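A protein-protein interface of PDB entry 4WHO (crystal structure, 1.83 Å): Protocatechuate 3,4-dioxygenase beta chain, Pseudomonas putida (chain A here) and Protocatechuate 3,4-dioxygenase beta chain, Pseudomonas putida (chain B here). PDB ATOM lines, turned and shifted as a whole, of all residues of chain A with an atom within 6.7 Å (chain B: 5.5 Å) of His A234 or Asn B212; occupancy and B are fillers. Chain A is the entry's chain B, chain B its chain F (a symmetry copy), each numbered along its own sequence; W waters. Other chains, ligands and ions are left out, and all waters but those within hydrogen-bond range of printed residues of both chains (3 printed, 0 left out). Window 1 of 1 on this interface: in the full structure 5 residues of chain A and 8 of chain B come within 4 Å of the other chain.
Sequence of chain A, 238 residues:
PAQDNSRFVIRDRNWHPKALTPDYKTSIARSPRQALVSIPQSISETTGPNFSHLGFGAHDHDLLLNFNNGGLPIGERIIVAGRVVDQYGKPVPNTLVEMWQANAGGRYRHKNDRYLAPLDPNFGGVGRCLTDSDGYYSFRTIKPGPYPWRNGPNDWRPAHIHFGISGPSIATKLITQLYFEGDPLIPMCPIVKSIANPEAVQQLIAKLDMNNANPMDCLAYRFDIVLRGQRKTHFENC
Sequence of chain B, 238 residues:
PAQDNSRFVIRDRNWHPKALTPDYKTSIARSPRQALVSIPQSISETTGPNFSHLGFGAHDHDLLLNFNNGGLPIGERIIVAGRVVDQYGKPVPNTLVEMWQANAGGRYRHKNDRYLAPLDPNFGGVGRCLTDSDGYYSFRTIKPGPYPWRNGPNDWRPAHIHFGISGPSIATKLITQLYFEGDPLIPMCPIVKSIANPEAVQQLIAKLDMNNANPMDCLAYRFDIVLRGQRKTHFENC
NE of Arg A231 is in hydrogen-bond range of O of Asn B211, at 3.2 Å. The guanidinium group of Arg A231 lies within hydrogen-bond range of the backbone carbonyl oxygen of Ala B213 (3.0 Å). The guanidinium group (NH2) of Arg A231 sits at hydrogen-bond distance from the side-chain amide oxygen (OD1) of Asn B214, at 3.1 Å. A ring nitrogen (NE2) of His A234 lies within hydrogen-bond range of the side-chain amide oxygen (OD1) of Asn B212, 3.1 Å away. O of His A234 is in hydrogen-bond range of ND2 of Asn B214 (2.8 Å).
The backbone carbonyl oxygen (O) of Arg A231 is in hydrogen-bond range of the backbone NH (N) of Arg A7. The backbone NH (N) of Ile B79 is in hydrogen-bond range of the backbone carbonyl oxygen (O) of Leu B219 (2.9 Å). ND2 of Asn B211 sits at hydrogen-bond distance from OD1 of Asp B209 (3.0 Å). The side-chain amide nitrogen (ND2) of Asn B212 sits close to the guanidinium group (NH2) of Arg B222 (3.5 Å).
Among the printed residues, merely in contact across the chains: Arg A231 with Asn B212, His A234 with Ile B79, Phe A235 with Asn B214, Val A9 with Asn B211, Phe A235 with Ile B79 and Tyr A88 with Asn B211.
Of chain B, only Ile B79 (3.5 Å), Asn B212 (2.9 Å) and Asn B214 (2.8 Å) come within 4 Å of His A234. Asn B212 touches just these residues of chain A: Arg A231 and His A234. Of the printed residues of chain A, Ile B79 touches His A234 (3.5 Å) and Phe A235 (3.7 Å). Printed residues of chain B within 4 Å of Arg A231: Asn B211, Asn B212, Ala B213 and Asn B214. Of the printed residues of chain A, Asn B214 touches Arg A231 (3.1 Å), His A234 (2.8 Å) and Phe A235 (3.5 Å). Of the printed residues of chain B, Phe A235 touches Ile B79 (3.7 Å) and Asn B214 (3.5 Å). Printed residues of chain A within 4 Å of Ala B213: Arg A231 (3.0 Å). Lys A232 touches none of the printed residues of chain B. Arg B222 touches none of the printed residues of chain A. The nearest residue of chain B that does not touch His A234 is Ala B213 (4.8 Å). The nearest residue of chain A that does not touch Asn B212 is Tyr A88 (5.1 Å).
Of the 9 printed residues of chain A, 5 touch a printed residue of chain B. Of the 12 printed residues of chain B, 5 touch a printed residue of chain A. Hydrophobic or aromatic side chains of chain B that line the printed part of chain A: Ile B79.
Water W3 lies within hydrogen-bond range of the side-chain hydroxyl of Tyr A88 (2.7 Å) and the side-chain amide oxygen of Asn B212 (2.9 Å). Water W1 lies within hydrogen-bond range of the side-chain amide oxygen of Asn B214 (2.7 Å), the side-chain carboxylate of Glu A236 (2.8 Å), the guanidinium group of Arg A231 (2.9 Å) and the backbone NH of His A234 (3.0 Å). Water W2 lies within hydrogen-bond range of O of Phe A235 (2.8 Å) and SG of Cys B218 (3.5 Å).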
ATOM      1  N   ARG A   7      20.954   6.888  22.805  1.00  0.00           N
ATOM      2  CA  ARG A   7      21.319   8.200  23.309  1.00  0.00           C
ATOM      3  C   ARG A   7      21.645   9.086  22.130  1.00  0.00           C
ATOM      4  O   ARG A   7      22.164   8.633  21.102  1.00  0.00           O
ATOM      5  CB  ARG A   7      22.526   8.108  24.249  1.00  0.00           C
ATOM      6  CG  ARG A   7      22.265   7.317  25.507  1.00  0.00           C
ATOM      7  CD  ARG A   7      21.359   8.052  26.487  1.00  0.00           C
ATOM      8  NE  ARG A   7      20.922   7.211  27.605  1.00  0.00           N
ATOM      9  CZ  ARG A   7      19.743   6.594  27.696  1.00  0.00           C
ATOM     10  NH1 ARG A   7      18.841   6.692  26.727  1.00  0.00           N
ATOM     11  NH2 ARG A   7      19.452   5.874  28.771  1.00  0.00           N
ATOM     12  N   VAL A   9      23.587  12.645  20.801  1.00  0.00           N
ATOM     13  CA  VAL A   9      24.694  13.546  21.048  1.00  0.00           C
ATOM     14  C   VAL A   9      24.136  14.911  21.470  1.00  0.00           C
ATOM     15  O   VAL A   9      23.163  15.410  20.904  1.00  0.00           O
ATOM     16  CB  VAL A   9      25.578  13.680  19.788  1.00  0.00           C
ATOM     17  CG1 VAL A   9      26.631  14.764  19.989  1.00  0.00           C
ATOM     18  CG2 VAL A   9      26.236  12.333  19.501  1.00  0.00           C
ATOM     19  N   TYR A  88      26.884  10.857  12.937  1.00  0.00           N
ATOM     20  CA  TYR A  88      27.784   9.774  12.666  1.00  0.00           C
ATOM     21  C   TYR A  88      27.781   9.368  11.204  1.00  0.00           C
ATOM     22  O   TYR A  88      28.524   8.479  10.841  1.00  0.00           O
ATOM     23  CB  TYR A  88      27.423   8.552  13.494  1.00  0.00           C
ATOM     24  CG  TYR A  88      27.547   8.753  14.978  1.00  0.00           C
ATOM     25  CD1 TYR A  88      28.786   8.778  15.586  1.00  0.00           C
ATOM     26  CD2 TYR A  88      26.409   8.884  15.777  1.00  0.00           C
ATOM     27  CE1 TYR A  88      28.899   8.934  16.975  1.00  0.00           C
ATOM     28  CE2 TYR A  88      26.515   9.071  17.140  1.00  0.00           C
ATOM     29  CZ  TYR A  88      27.745   9.068  17.733  1.00  0.00           C
ATOM     30  OH  TYR A  88      27.819   9.263  19.091  1.00  0.00           O
ATOM     31  N   ARG A 231      23.512   6.882  19.214  1.00  0.00           N
ATOM     32  CA  ARG A 231      24.313   5.708  19.641  1.00  0.00           C
ATOM     33  C   ARG A 231      23.527   4.817  20.597  1.00  0.00           C
ATOM     34  O   ARG A 231      22.605   5.274  21.269  1.00  0.00           O
ATOM     35  CB  ARG A 231      25.637   6.151  20.290  1.00  0.00           C
ATOM     36  CG  ARG A 231      25.519   6.765  21.688  1.00  0.00           C
ATOM     37  CD  ARG A 231      26.876   6.901  22.352  1.00  0.00           C
ATOM     38  NE  ARG A 231      26.872   7.626  23.610  1.00  0.00           N
ATOM     39  CZ  ARG A 231      26.379   7.183  24.760  1.00  0.00           C
ATOM     40  NH1 ARG A 231      25.821   5.983  24.842  1.00  0.00           N
ATOM     41  NH2 ARG A 231      26.500   7.928  25.861  1.00  0.00           N
ATOM     42  N   LYS A 232      23.910   3.543  20.687  1.00  0.00           N
ATOM     43  CA  LYS A 232      23.372   2.689  21.721  1.00  0.00           C
ATOM     44  C   LYS A 232      23.814   3.147  23.106  1.00  0.00           C
ATOM     45  O   LYS A 232      24.927   3.635  23.280  1.00  0.00           O
ATOM     46  CB  LYS A 232      23.846   1.246  21.508  1.00  0.00           C
ATOM     47  CG  LYS A 232      23.303   0.642  20.243  1.00  0.00           C
ATOM     48  CD  LYS A 232      23.973  -0.696  19.950  1.00  0.00           C
ATOM     49  CE  LYS A 232      23.451  -1.269  18.629  1.00  0.00           C
ATOM     50  NZ  LYS A 232      23.522  -2.765  18.646  1.00  0.00           N
ATOM     51  N   THR A 233      22.954   2.975  24.100  1.00  0.00           N
ATOM     52  CA  THR A 233      23.374   3.115  25.514  1.00  0.00           C
ATOM     53  C   THR A 233      24.514   2.146  25.824  1.00  0.00           C
ATOM     54  O   THR A 233      24.578   1.042  25.267  1.00  0.00           O
ATOM     55  CB  THR A 233      22.222   2.765  26.449  1.00  0.00           C
ATOM     56  OG1 THR A 233      21.806   1.428  26.150  1.00  0.00           O
ATOM     57  CG2 THR A 233      21.073   3.671  26.233  1.00  0.00           C
ATOM     58  N   HIS A 234      25.427   2.548  26.691  1.00  0.00           N
ATOM     59  CA  HIS A 234      26.468   1.650  27.150  1.00  0.00           C
ATOM     60  C   HIS A 234      26.802   1.975  28.594  1.00  0.00           C
ATOM     61  O   HIS A 234      26.770   3.132  28.996  1.00  0.00           O
ATOM     62  CB  HIS A 234      27.713   1.684  26.223  1.00  0.00           C
ATOM     63  CG  HIS A 234      28.235   3.058  25.867  1.00  0.00           C
ATOM     64  ND1 HIS A 234      28.301   4.114  26.755  1.00  0.00           N
ATOM     65  CD2 HIS A 234      28.811   3.506  24.723  1.00  0.00           C
ATOM     66  CE1 HIS A 234      28.839   5.165  26.162  1.00  0.00           C
ATOM     67  NE2 HIS A 234      29.150   4.826  24.923  1.00  0.00           N
ATOM     68  N   PHE A 235      27.130   0.934  29.358  1.00  0.00           N
ATOM     69  CA  PHE A 235      27.664   1.063  30.714  1.00  0.00           C
ATOM     70  C   PHE A 235      26.785   1.891  31.669  1.00  0.00           C
ATOM     71  O   PHE A 235      27.309   2.605  32.516  1.00  0.00           O
ATOM     72  CB  PHE A 235      29.089   1.649  30.692  1.00  0.00           C
ATOM     73  CG  PHE A 235      30.100   0.793  29.980  1.00  0.00           C
ATOM     74  CD1 PHE A 235      30.522  -0.419  30.530  1.00  0.00           C
ATOM     75  CD2 PHE A 235      30.619   1.180  28.761  1.00  0.00           C
ATOM     76  CE1 PHE A 235      31.455  -1.207  29.871  1.00  0.00           C
ATOM     77  CE2 PHE A 235      31.553   0.400  28.101  1.00  0.00           C
ATOM     78  CZ  PHE A 235      31.965  -0.803  28.657  1.00  0.00           C
ATOM     79  N   GLU A 236      25.466   1.842  31.500  1.00  0.00           N
ATOM     80  CA  GLU A 236      24.541   2.580  32.361  1.00  0.00           C
ATOM     81  C   GLU A 236      24.027   1.726  33.542  1.00  0.00           C
ATOM     82  O   GLU A 236      23.822   0.528  33.355  1.00  0.00           O
ATOM     83  CB  GLU A 236      23.374   3.128  31.521  1.00  0.00           C
ATOM     84  CG  GLU A 236      23.829   4.315  30.652  1.00  0.00           C
ATOM     85  CD  GLU A 236      22.672   5.097  30.042  1.00  0.00           C
ATOM     86  OE1 GLU A 236      21.528   4.950  30.513  1.00  0.00           O
ATOM     87  OE2 GLU A 236      22.905   5.883  29.106  1.00  0.00           O
ATOM     88  N   ILE B  79      35.573   5.378  29.438  1.00  0.00           N
ATOM     89  CA  ILE B  79      35.357   4.375  28.456  1.00  0.00           C
ATOM     90  C   ILE B  79      36.464   4.525  27.397  1.00  0.00           C
ATOM     91  O   ILE B  79      36.775   5.636  26.964  1.00  0.00           O
ATOM     92  CB  ILE B  79      33.973   4.531  27.783  1.00  0.00           C
ATOM     93  CG1 ILE B  79      32.851   4.227  28.799  1.00  0.00           C
ATOM     94  CG2 ILE B  79      33.926   3.702  26.505  1.00  0.00           C
ATOM     95  CD1 ILE B  79      31.482   4.762  28.393  1.00  0.00           C
ATOM     96  N   ALA B  81      37.236   3.119  23.696  1.00  0.00           N
ATOM     97  CA  ALA B  81      36.530   2.429  22.608  1.00  0.00           C
ATOM     98  C   ALA B  81      37.117   2.785  21.263  1.00  0.00           C
ATOM     99  O   ALA B  81      37.755   3.838  21.091  1.00  0.00           O
ATOM    100  CB  ALA B  81      35.048   2.794  22.658  1.00  0.00           C
ATOM    101  N   ASP B 209      36.588  11.902  23.548  1.00  0.00           N
ATOM    102  CA  ASP B 209      35.403  11.577  22.763  1.00  0.00           C
ATOM    103  C   ASP B 209      34.162  11.877  23.589  1.00  0.00           C
ATOM    104  O   ASP B 209      33.542  10.985  24.184  1.00  0.00           O
ATOM    105  CB  ASP B 209      35.427  10.100  22.349  1.00  0.00           C
ATOM    106  CG  ASP B 209      34.353   9.731  21.342  1.00  0.00           C
ATOM    107  OD1 ASP B 209      33.587  10.610  20.883  1.00  0.00           O
ATOM    108  OD2 ASP B 209      34.288   8.521  21.007  1.00  0.00           O
ATOM    109  N   MET B 210      33.776  13.145  23.591  1.00  0.00           N
ATOM    110  CA  MET B 210      32.649  13.587  24.448  1.00  0.00           C
ATOM    111  C   MET B 210      31.336  12.945  24.022  1.00  0.00           C
ATOM    112  O   MET B 210      30.430  12.801  24.829  1.00  0.00           O
ATOM    113  CB  MET B 210      32.504  15.105  24.410  1.00  0.00           C
ATOM    114  CG  MET B 210      33.751  15.810  24.833  1.00  0.00           C
ATOM    115  SD  MET B 210      34.214  15.449  26.524  1.00  0.00           S
ATOM    116  CE  MET B 210      32.895  16.132  27.521  1.00  0.00           C
ATOM    117  N   ASN B 211      31.233  12.587  22.739  1.00  0.00           N
ATOM    118  CA  ASN B 211      30.060  11.972  22.154  1.00  0.00           C
ATOM    119  C   ASN B 211      29.798  10.599  22.759  1.00  0.00           C
ATOM    120  O   ASN B 211      28.664  10.108  22.840  1.00  0.00           O
ATOM    121  CB  ASN B 211      30.228  11.857  20.594  1.00  0.00           C
ATOM    122  CG  ASN B 211      30.873  13.080  19.981  1.00  0.00           C
ATOM    123  OD1 ASN B 211      30.235  14.116  19.802  1.00  0.00           O
ATOM    124  ND2 ASN B 211      32.169  12.980  19.688  1.00  0.00           N
ATOM    125  N   ASN B 212      30.849   9.966  23.231  1.00  0.00           N
ATOM    126  CA  ASN B 212      30.723   8.630  23.793  1.00  0.00           C
ATOM    127  C   ASN B 212      30.638   8.616  25.309  1.00  0.00           C
ATOM    128  O   ASN B 212      30.513   7.578  25.929  1.00  0.00           O
ATOM    129  CB  ASN B 212      31.881   7.747  23.316  1.00  0.00           C
ATOM    130  CG  ASN B 212      31.402   6.403  22.793  1.00  0.00           C
ATOM    131  OD1 ASN B 212      30.252   6.284  22.381  1.00  0.00           O
ATOM    132  ND2 ASN B 212      32.279   5.392  22.816  1.00  0.00           N
ATOM    133  N   ALA B 213      30.734   9.773  25.921  1.00  0.00           N
ATOM    134  CA  ALA B 213      30.743   9.875  27.361  1.00  0.00           C
ATOM    135  C   ALA B 213      29.353   9.619  27.897  1.00  0.00           C
ATOM    136  O   ALA B 213      28.380   9.847  27.168  1.00  0.00           O
ATOM    137  CB  ALA B 213      31.207  11.250  27.766  1.00  0.00           C
ATOM    138  N   ASN B 214      29.273   9.178  29.165  1.00  0.00           N
ATOM    139  CA  ASN B 214      28.031   9.112  29.918  1.00  0.00           C
ATOM    140  C   ASN B 214      27.969  10.324  30.842  1.00  0.00           C
ATOM    141  O   ASN B 214      28.704  10.420  31.791  1.00  0.00           O
ATOM    142  CB  ASN B 214      27.876   7.811  30.718  1.00  0.00           C
ATOM    143  CG  ASN B 214      27.532   6.604  29.848  1.00  0.00           C
ATOM    144  OD1 ASN B 214      27.144   6.757  28.708  1.00  0.00           O
ATOM    145  ND2 ASN B 214      27.678   5.397  30.393  1.00  0.00           N
ATOM    146  N   CYS B 218      30.956   9.022  33.312  1.00  0.00           N
ATOM    147  CA  CYS B 218      32.300   8.765  32.831  1.00  0.00           C
ATOM    148  C   CYS B 218      32.628   9.465  31.499  1.00  0.00           C
ATOM    149  O   CYS B 218      31.760   9.652  30.644  1.00  0.00           O
ATOM    150  CB  CYS B 218      32.500   7.257  32.699  1.00  0.00           C
ATOM    151  SG  CYS B 218      31.553   6.511  31.370  1.00  0.00           S
ATOM    152  N   LEU B 219      33.894   9.848  31.338  1.00  0.00           N
ATOM    153  CA  LEU B 219      34.371  10.388  30.069  1.00  0.00           C
ATOM    154  C   LEU B 219      34.678   9.262  29.119  1.00  0.00           C
ATOM    155  O   LEU B 219      34.415   8.079  29.430  1.00  0.00           O
ATOM    156  CB  LEU B 219      35.585  11.290  30.301  1.00  0.00           C
ATOM    157  CG  LEU B 219      35.127  12.678  30.766  1.00  0.00           C
ATOM    158  CD1 LEU B 219      36.334  13.421  31.320  1.00  0.00           C
ATOM    159  CD2 LEU B 219      34.406  13.452  29.660  1.00  0.00           C
ATOM    160  N   ALA B 220      35.155   9.593  27.932  1.00  0.00           N
ATOM    161  CA  ALA B 220      35.471   8.551  26.952  1.00  0.00           C
ATOM    162  C   ALA B 220      36.575   9.024  26.055  1.00  0.00           C
ATOM    163  O   ALA B 220      36.708  10.232  25.795  1.00  0.00           O
ATOM    164  CB  ALA B 220      34.261   8.141  26.125  1.00  0.00           C
ATOM    165  N   ARG B 222      38.758   7.721  22.328  1.00  0.00           N
ATOM    166  CA  ARG B 222      38.622   6.906  21.127  1.00  0.00           C
ATOM    167  C   ARG B 222      40.009   6.507  20.584  1.00  0.00           C
ATOM    168  O   ARG B 222      40.870   7.358  20.442  1.00  0.00           O
ATOM    169  CB  ARG B 222      37.823   7.704  20.101  1.00  0.00           C
ATOM    170  CG  ARG B 222      37.782   7.109  18.694  1.00  0.00           C
ATOM    171  CD  ARG B 222      36.536   6.373  18.282  1.00  0.00           C
ATOM    172  NE  ARG B 222      35.273   6.690  18.960  1.00  0.00           N
ATOM    173  CZ  ARG B 222      34.193   5.900  18.870  1.00  0.00           C
ATOM    174  NH1 ARG B 222      34.215   4.815  18.100  1.00  0.00           N
ATOM    175  NH2 ARG B 222      33.081   6.193  19.536  1.00  0.00           N
HETATM  176  O   HOH W   1      25.120   5.377  27.547  1.00  0.00           O
HETATM  177  O   HOH W   2      29.648   4.108  33.129  1.00  0.00           O
HETATM  178  O   HOH W   3      29.911   7.880  19.991  1.00  0.00           O
